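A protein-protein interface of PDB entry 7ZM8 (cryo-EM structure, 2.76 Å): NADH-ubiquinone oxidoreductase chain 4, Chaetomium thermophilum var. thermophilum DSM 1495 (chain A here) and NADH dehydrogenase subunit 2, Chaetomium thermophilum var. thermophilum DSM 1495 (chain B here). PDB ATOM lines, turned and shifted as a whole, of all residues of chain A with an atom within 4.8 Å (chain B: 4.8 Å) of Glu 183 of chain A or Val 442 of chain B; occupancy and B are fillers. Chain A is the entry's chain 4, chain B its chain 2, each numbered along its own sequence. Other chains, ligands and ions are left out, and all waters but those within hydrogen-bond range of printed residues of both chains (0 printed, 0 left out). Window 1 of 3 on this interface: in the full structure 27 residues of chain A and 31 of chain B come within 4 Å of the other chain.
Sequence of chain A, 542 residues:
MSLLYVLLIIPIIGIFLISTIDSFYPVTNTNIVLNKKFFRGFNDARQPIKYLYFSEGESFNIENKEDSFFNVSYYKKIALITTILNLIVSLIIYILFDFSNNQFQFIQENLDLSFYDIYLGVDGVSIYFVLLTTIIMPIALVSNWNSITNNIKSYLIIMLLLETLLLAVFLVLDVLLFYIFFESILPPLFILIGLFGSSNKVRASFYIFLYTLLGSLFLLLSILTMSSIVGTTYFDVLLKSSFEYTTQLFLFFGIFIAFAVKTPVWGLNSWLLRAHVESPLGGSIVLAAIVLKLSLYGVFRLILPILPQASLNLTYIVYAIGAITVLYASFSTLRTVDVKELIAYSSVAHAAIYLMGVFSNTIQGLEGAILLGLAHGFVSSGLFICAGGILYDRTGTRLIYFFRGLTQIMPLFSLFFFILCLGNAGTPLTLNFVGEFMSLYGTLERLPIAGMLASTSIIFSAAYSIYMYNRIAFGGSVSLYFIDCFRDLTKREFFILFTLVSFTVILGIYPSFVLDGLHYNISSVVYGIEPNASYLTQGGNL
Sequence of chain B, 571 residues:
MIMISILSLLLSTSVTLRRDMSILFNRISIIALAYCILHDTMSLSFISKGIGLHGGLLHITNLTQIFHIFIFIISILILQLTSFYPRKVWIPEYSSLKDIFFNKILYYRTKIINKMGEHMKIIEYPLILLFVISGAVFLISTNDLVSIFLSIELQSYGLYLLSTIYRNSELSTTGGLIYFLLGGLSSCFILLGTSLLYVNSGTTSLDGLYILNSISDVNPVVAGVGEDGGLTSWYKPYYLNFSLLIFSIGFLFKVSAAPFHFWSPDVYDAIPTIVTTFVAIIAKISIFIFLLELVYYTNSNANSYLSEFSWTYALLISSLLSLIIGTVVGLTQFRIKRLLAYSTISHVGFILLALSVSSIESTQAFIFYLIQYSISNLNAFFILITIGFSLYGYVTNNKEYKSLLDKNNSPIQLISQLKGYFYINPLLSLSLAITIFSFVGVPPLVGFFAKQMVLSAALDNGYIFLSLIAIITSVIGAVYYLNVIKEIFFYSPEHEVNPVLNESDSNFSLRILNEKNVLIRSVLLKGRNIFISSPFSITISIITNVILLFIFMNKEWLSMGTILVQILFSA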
ATOM      1  N   TYR A 179      34.390   5.616 -11.265  1.00  0.00           N
ATOM      2  CA  TYR A 179      33.654   5.616 -10.006  1.00  0.00           C
ATOM      3  C   TYR A 179      32.257   6.191 -10.185  1.00  0.00           C
ATOM      4  O   TYR A 179      31.304   5.747  -9.540  1.00  0.00           O
ATOM      5  CB  TYR A 179      34.437   6.405  -8.952  1.00  0.00           C
ATOM      6  CG  TYR A 179      33.708   6.572  -7.639  1.00  0.00           C
ATOM      7  CD1 TYR A 179      32.834   7.630  -7.437  1.00  0.00           C
ATOM      8  CD2 TYR A 179      33.885   5.670  -6.609  1.00  0.00           C
ATOM      9  CE1 TYR A 179      32.161   7.776  -6.264  1.00  0.00           C
ATOM     10  CE2 TYR A 179      33.218   5.819  -5.426  1.00  0.00           C
ATOM     11  CZ  TYR A 179      32.357   6.873  -5.259  1.00  0.00           C
ATOM     12  OH  TYR A 179      31.684   7.029  -4.075  1.00  0.00           O
ATOM     13  N   ILE A 180      32.121   7.192 -11.055  1.00  0.00           N
ATOM     14  CA  ILE A 180      30.840   7.869 -11.230  1.00  0.00           C
ATOM     15  C   ILE A 180      29.778   6.895 -11.718  1.00  0.00           C
ATOM     16  O   ILE A 180      28.644   6.894 -11.227  1.00  0.00           O
ATOM     17  CB  ILE A 180      30.997   9.068 -12.184  1.00  0.00           C
ATOM     18  CG1 ILE A 180      31.655  10.243 -11.462  1.00  0.00           C
ATOM     19  CG2 ILE A 180      29.654   9.471 -12.761  1.00  0.00           C
ATOM     20  CD1 ILE A 180      32.293  11.236 -12.381  1.00  0.00           C
ATOM     21  N   PHE A 181      30.128   6.046 -12.683  1.00  0.00           N
ATOM     22  CA  PHE A 181      29.172   5.081 -13.210  1.00  0.00           C
ATOM     23  C   PHE A 181      29.168   3.780 -12.417  1.00  0.00           C
ATOM     24  O   PHE A 181      28.150   3.084 -12.376  1.00  0.00           O
ATOM     25  CB  PHE A 181      29.466   4.825 -14.680  1.00  0.00           C
ATOM     26  CG  PHE A 181      29.372   6.053 -15.516  1.00  0.00           C
ATOM     27  CD1 PHE A 181      28.208   6.793 -15.530  1.00  0.00           C
ATOM     28  CD2 PHE A 181      30.443   6.491 -16.259  1.00  0.00           C
ATOM     29  CE1 PHE A 181      28.112   7.932 -16.278  1.00  0.00           C
ATOM     30  CE2 PHE A 181      30.343   7.626 -17.005  1.00  0.00           C
ATOM     31  CZ  PHE A 181      29.177   8.348 -17.014  1.00  0.00           C
ATOM     32  N   PHE A 182      30.297   3.430 -11.799  1.00  0.00           N
ATOM     33  CA  PHE A 182      30.375   2.209 -10.953  1.00  0.00           C
ATOM     34  C   PHE A 182      29.424   2.381  -9.773  1.00  0.00           C
ATOM     35  O   PHE A 182      29.111   1.381  -9.113  1.00  0.00           O
ATOM     36  CB  PHE A 182      31.825   1.962 -10.520  1.00  0.00           C
ATOM     37  CG  PHE A 182      32.067   0.894  -9.483  1.00  0.00           C
ATOM     38  CD1 PHE A 182      32.267   1.228  -8.154  1.00  0.00           C
ATOM     39  CD2 PHE A 182      32.142  -0.442  -9.840  1.00  0.00           C
ATOM     40  CE1 PHE A 182      32.501   0.248  -7.201  1.00  0.00           C
ATOM     41  CE2 PHE A 182      32.380  -1.420  -8.888  1.00  0.00           C
ATOM     42  CZ  PHE A 182      32.558  -1.074  -7.571  1.00  0.00           C
ATOM     43  N   GLU A 183      28.934   3.602  -9.551  1.00  0.00           N
ATOM     44  CA  GLU A 183      28.083   3.864  -8.359  1.00  0.00           C
ATOM     45  C   GLU A 183      26.793   4.583  -8.746  1.00  0.00           C
ATOM     46  O   GLU A 183      25.989   4.841  -7.837  1.00  0.00           O
ATOM     47  CB  GLU A 183      28.850   4.675  -7.314  1.00  0.00           C
ATOM     48  CG  GLU A 183      29.749   3.809  -6.458  1.00  0.00           C
ATOM     49  CD  GLU A 183      29.060   2.569  -5.912  1.00  0.00           C
ATOM     50  OE1 GLU A 183      28.039   2.720  -5.213  1.00  0.00           O
ATOM     51  OE2 GLU A 183      29.546   1.454  -6.187  1.00  0.00           O
ATOM     52  N   SER A 184      26.584   4.902 -10.017  1.00  0.00           N
ATOM     53  CA  SER A 184      25.338   5.504 -10.461  1.00  0.00           C
ATOM     54  C   SER A 184      24.230   4.478 -10.610  1.00  0.00           C
ATOM     55  O   SER A 184      23.075   4.858 -10.819  1.00  0.00           O
ATOM     56  CB  SER A 184      25.537   6.241 -11.788  1.00  0.00           C
ATOM     57  OG  SER A 184      25.869   5.343 -12.825  1.00  0.00           O
ATOM     58  N   ILE A 185      24.550   3.213 -10.379  1.00  0.00           N
ATOM     59  CA  ILE A 185      23.652   2.072 -10.701  1.00  0.00           C
ATOM     60  C   ILE A 185      22.908   1.768  -9.412  1.00  0.00           C
ATOM     61  O   ILE A 185      21.963   0.972  -9.449  1.00  0.00           O
ATOM     62  CB  ILE A 185      24.477   0.866 -11.187  1.00  0.00           C
ATOM     63  CG1 ILE A 185      25.458   0.387 -10.118  1.00  0.00           C
ATOM     64  CG2 ILE A 185      25.183   1.181 -12.497  1.00  0.00           C
ATOM     65  CD1 ILE A 185      26.168  -0.887 -10.476  1.00  0.00           C
ATOM     66  N   LEU A 186      23.303   2.427  -8.327  1.00  0.00           N
ATOM     67  CA  LEU A 186      22.774   2.068  -6.992  1.00  0.00           C
ATOM     68  C   LEU A 186      21.349   2.623  -6.853  1.00  0.00           C
ATOM     69  O   LEU A 186      20.507   1.872  -6.342  1.00  0.00           O
ATOM     70  CB  LEU A 186      23.733   2.645  -5.946  1.00  0.00           C
ATOM     71  CG  LEU A 186      23.856   1.845  -4.652  1.00  0.00           C
ATOM     72  CD1 LEU A 186      24.002   0.360  -4.942  1.00  0.00           C
ATOM     73  CD2 LEU A 186      25.016   2.354  -3.814  1.00  0.00           C
ATOM     74  N   PRO A 187      20.997   3.874  -7.257  1.00  0.00           N
ATOM     75  CA  PRO A 187      19.587   4.303  -7.200  1.00  0.00           C
ATOM     76  C   PRO A 187      18.578   3.514  -8.051  1.00  0.00           C
ATOM     77  O   PRO A 187      17.529   3.210  -7.517  1.00  0.00           O
ATOM     78  CB  PRO A 187      19.619   5.785  -7.599  1.00  0.00           C
ATOM     79  CG  PRO A 187      21.029   6.200  -7.298  1.00  0.00           C
ATOM     80  CD  PRO A 187      21.867   4.988  -7.644  1.00  0.00           C
ATOM     81  N   PHE A 209      22.215  -1.295  -1.220  1.00  0.00           N
ATOM     82  CA  PHE A 209      22.579   0.124  -1.380  1.00  0.00           C
ATOM     83  C   PHE A 209      23.615   0.498  -0.323  1.00  0.00           C
ATOM     84  O   PHE A 209      24.657   1.012  -0.712  1.00  0.00           O
ATOM     85  CB  PHE A 209      21.350   1.037  -1.271  1.00  0.00           C
ATOM     86  CG  PHE A 209      21.573   2.479  -1.657  1.00  0.00           C
ATOM     87  CD1 PHE A 209      22.248   3.354  -0.819  1.00  0.00           C
ATOM     88  CD2 PHE A 209      21.089   2.971  -2.856  1.00  0.00           C
ATOM     89  CE1 PHE A 209      22.448   4.676  -1.176  1.00  0.00           C
ATOM     90  CE2 PHE A 209      21.286   4.294  -3.214  1.00  0.00           C
ATOM     91  CZ  PHE A 209      21.969   5.143  -2.375  1.00  0.00           C
ATOM     92  N   THR A 212      27.106  -1.219  -0.634  1.00  0.00           N
ATOM     93  CA  THR A 212      27.792  -0.765  -1.869  1.00  0.00           C
ATOM     94  C   THR A 212      28.138   0.709  -1.715  1.00  0.00           C
ATOM     95  O   THR A 212      29.170   1.121  -2.249  1.00  0.00           O
ATOM     96  CB  THR A 212      26.944  -1.052  -3.114  1.00  0.00           C
ATOM     97  OG1 THR A 212      26.628  -2.444  -3.122  1.00  0.00           O
ATOM     98  CG2 THR A 212      27.626  -0.677  -4.410  1.00  0.00           C
ATOM     99  N   LEU A 213      27.304   1.464  -1.002  1.00  0.00           N
ATOM    100  CA  LEU A 213      27.668   2.852  -0.761  1.00  0.00           C
ATOM    101  C   LEU A 213      28.840   2.957   0.200  1.00  0.00           C
ATOM    102  O   LEU A 213      29.763   3.743  -0.029  1.00  0.00           O
ATOM    103  CB  LEU A 213      26.468   3.625  -0.211  1.00  0.00           C
ATOM    104  CG  LEU A 213      26.722   5.091   0.134  1.00  0.00           C
ATOM    105  CD1 LEU A 213      26.822   5.916  -1.121  1.00  0.00           C
ATOM    106  CD2 LEU A 213      25.663   5.622   1.069  1.00  0.00           C
ATOM    107  N   SER A 216      32.141   1.609  -1.419  1.00  0.00           N
ATOM    108  CA  SER A 216      32.626   2.425  -2.521  1.00  0.00           C
ATOM    109  C   SER A 216      33.141   3.782  -2.066  1.00  0.00           C
ATOM    110  O   SER A 216      33.807   4.465  -2.844  1.00  0.00           O
ATOM    111  CB  SER A 216      31.522   2.613  -3.557  1.00  0.00           C
ATOM    112  OG  SER A 216      30.512   3.480  -3.079  1.00  0.00           O
ATOM    113  N   PHE B 437      18.501  11.670  -3.330  1.00  0.00           N
ATOM    114  CA  PHE B 437      19.748  10.986  -3.642  1.00  0.00           C
ATOM    115  C   PHE B 437      20.906  11.967  -3.789  1.00  0.00           C
ATOM    116  O   PHE B 437      22.066  11.587  -3.614  1.00  0.00           O
ATOM    117  CB  PHE B 437      19.582  10.151  -4.910  1.00  0.00           C
ATOM    118  CG  PHE B 437      18.843   8.866  -4.699  1.00  0.00           C
ATOM    119  CD1 PHE B 437      19.301   7.925  -3.798  1.00  0.00           C
ATOM    120  CD2 PHE B 437      17.690   8.596  -5.410  1.00  0.00           C
ATOM    121  CE1 PHE B 437      18.619   6.746  -3.607  1.00  0.00           C
ATOM    122  CE2 PHE B 437      17.004   7.423  -5.222  1.00  0.00           C
ATOM    123  CZ  PHE B 437      17.468   6.493  -4.320  1.00  0.00           C
ATOM    124  N   VAL B 440      22.240  12.399  -0.363  1.00  0.00           N
ATOM    125  CA  VAL B 440      23.084  11.257  -0.026  1.00  0.00           C
ATOM    126  C   VAL B 440      24.475  11.420  -0.624  1.00  0.00           C
ATOM    127  O   VAL B 440      25.483  11.122   0.027  1.00  0.00           O
ATOM    128  CB  VAL B 440      22.421   9.949  -0.494  1.00  0.00           C
ATOM    129  CG1 VAL B 440      23.351   8.771  -0.270  1.00  0.00           C
ATOM    130  CG2 VAL B 440      21.124   9.734   0.229  1.00  0.00           C
ATOM    131  N   GLY B 441      24.534  11.908  -1.860  1.00  0.00           N
ATOM    132  CA  GLY B 441      25.830  12.071  -2.535  1.00  0.00           C
ATOM    133  C   GLY B 441      26.014  11.010  -3.598  1.00  0.00           C
ATOM    134  O   GLY B 441      27.163  10.624  -3.844  1.00  0.00           O
ATOM    135  N   VAL B 442      24.958  10.608  -4.284  1.00  0.00           N
ATOM    136  CA  VAL B 442      25.104   9.501  -5.265  1.00  0.00           C
ATOM    137  C   VAL B 442      25.426  10.101  -6.639  1.00  0.00           C
ATOM    138  O   VAL B 442      24.723  11.009  -7.053  1.00  0.00           O
ATOM    139  CB  VAL B 442      23.859   8.595  -5.278  1.00  0.00           C
ATOM    140  CG1 VAL B 442      24.179   7.242  -5.887  1.00  0.00           C
ATOM    141  CG2 VAL B 442      23.273   8.419  -3.891  1.00  0.00           C
ATOM    142  N   PRO B 443      26.474   9.639  -7.353  1.00  0.00           N
ATOM    143  CA  PRO B 443      26.768  10.114  -8.712  1.00  0.00           C
ATOM    144  C   PRO B 443      25.732   9.597  -9.731  1.00  0.00           C
ATOM    145  O   PRO B 443      25.155   8.581  -9.461  1.00  0.00           O
ATOM    146  CB  PRO B 443      28.159   9.530  -9.001  1.00  0.00           C
ATOM    147  CG  PRO B 443      28.650   8.918  -7.710  1.00  0.00           C
ATOM    148  CD  PRO B 443      27.418   8.625  -6.891  1.00  0.00           C
ATOM    149  N   PRO B 444      25.394  10.300 -10.835  1.00  0.00           N
ATOM    150  CA  PRO B 444      26.112  11.494 -11.304  1.00  0.00           C
ATOM    151  C   PRO B 444      25.566  12.798 -10.713  1.00  0.00           C
ATOM    152  O   PRO B 444      25.948  13.813 -11.200  1.00  0.00           O
ATOM    153  CB  PRO B 444      25.841  11.440 -12.808  1.00  0.00           C
ATOM    154  CG  PRO B 444      24.447  10.880 -12.913  1.00  0.00           C
ATOM    155  CD  PRO B 444      24.294   9.950 -11.730  1.00  0.00           C
ATOM    156  N   LEU B 445      24.710  12.716  -9.693  1.00  0.00           N
ATOM    157  CA  LEU B 445      24.014  13.887  -9.096  1.00  0.00           C
ATOM    158  C   LEU B 445      24.959  14.957  -8.559  1.00  0.00           C
ATOM    159  O   LEU B 445      26.046  14.603  -8.097  1.00  0.00           O
ATOM    160  CB  LEU B 445      23.022  13.385  -8.049  1.00  0.00           C
ATOM    161  CG  LEU B 445      22.024  12.360  -8.586  1.00  0.00           C
ATOM    162  CD1 LEU B 445      21.020  11.968  -7.523  1.00  0.00           C
ATOM    163  CD2 LEU B 445      21.312  12.886  -9.822  1.00  0.00           C
ATOM    164  N   PHE B 448      26.908  14.850  -5.186  1.00  0.00           N
ATOM    165  CA  PHE B 448      28.109  14.034  -5.082  1.00  0.00           C
ATOM    166  C   PHE B 448      29.354  14.867  -5.324  1.00  0.00           C
ATOM    167  O   PHE B 448      30.331  14.781  -4.575  1.00  0.00           O
ATOM    168  CB  PHE B 448      28.064  12.888  -6.082  1.00  0.00           C
ATOM    169  CG  PHE B 448      29.420  12.331  -6.408  1.00  0.00           C
ATOM    170  CD1 PHE B 448      30.060  11.482  -5.528  1.00  0.00           C
ATOM    171  CD2 PHE B 448      30.062  12.672  -7.587  1.00  0.00           C
ATOM    172  CE1 PHE B 448      31.308  10.988  -5.816  1.00  0.00           C
ATOM    173  CE2 PHE B 448      31.304  12.178  -7.879  1.00  0.00           C
ATOM    174  CZ  PHE B 448      31.930  11.334  -6.995  1.00  0.00           C
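The backbone carbonyl oxygen (O) of Phe 181 of chain A lies within hydrogen-bond range of the side-chain hydroxyl (OG) of Ser 184 of chain A (3.2 Å). O of Phe 437 of chain B sits at hydrogen-bond distance from N of Val 442 of chain B, 3.1 Å away. The side-chain carboxylate of Glu 183 of chain A lies close to the side-chain hydroxyl of Ser 216 of chain A (3.4 Å).
Among the printed residues, pairs that only touch across the chains: Ser 184 of chain A with Pro 443 of chain B, Tyr 179 of chain A with Phe 448 of chain B, Ile 180 of chain A with Pro 443 of chain B, Glu 183 of chain A with Val 442 of chain B, Pro 187 of chain A with Val 442 of chain B, Phe 209 of chain A with Phe 437 of chain B, Phe 209 of chain A with Val 442 of chain B, Pro 187 of chain A with Phe 437 of chain B, Ser 184 of chain A with Pro 444 of chain B and Tyr 179 of chain A with Pro 443 of chain B.
Of the printed residues of chain B, Tyr 179 of chain A touches Pro 443 and Phe 448. Of the printed residues of chain B, Ile 180 of chain A touches Pro 443 (3.5 Å). Phe 181 of chain A touches none of the printed residues of chain B. Of chain B, only Val 442 comes within 4 Å of Glu 183 of chain A. Of the printed residues of chain A, Phe 437 of chain B touches Pro 187 (3.9 Å) and Phe 209 (3.6 Å). Of chain A, only Glu 183, Pro 187 and Phe 209 come within 4 Å of Val 442 of chain B. Printed residues of chain A within 4 Å of Pro 443 of chain B: Tyr 179, Ile 180 and Ser 184. The nearest residue of chain B that does not touch Glu 183 of chain A is Pro 443 of chain B (4.2 Å). The nearest printed residue of chain B that does not touch Ser 184 of chain A is Val 442 of chain B (5.0 Å).
Hydrophobic or aromatic side chains of chain A within 4 Å of the printed part of chain B: Tyr 179, Pro 187 and Phe 209. Among the printed residues, no Asp or Glu carboxylate lies within 4 Å of a Lys or Arg side-chain nitrogen of the other chain.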
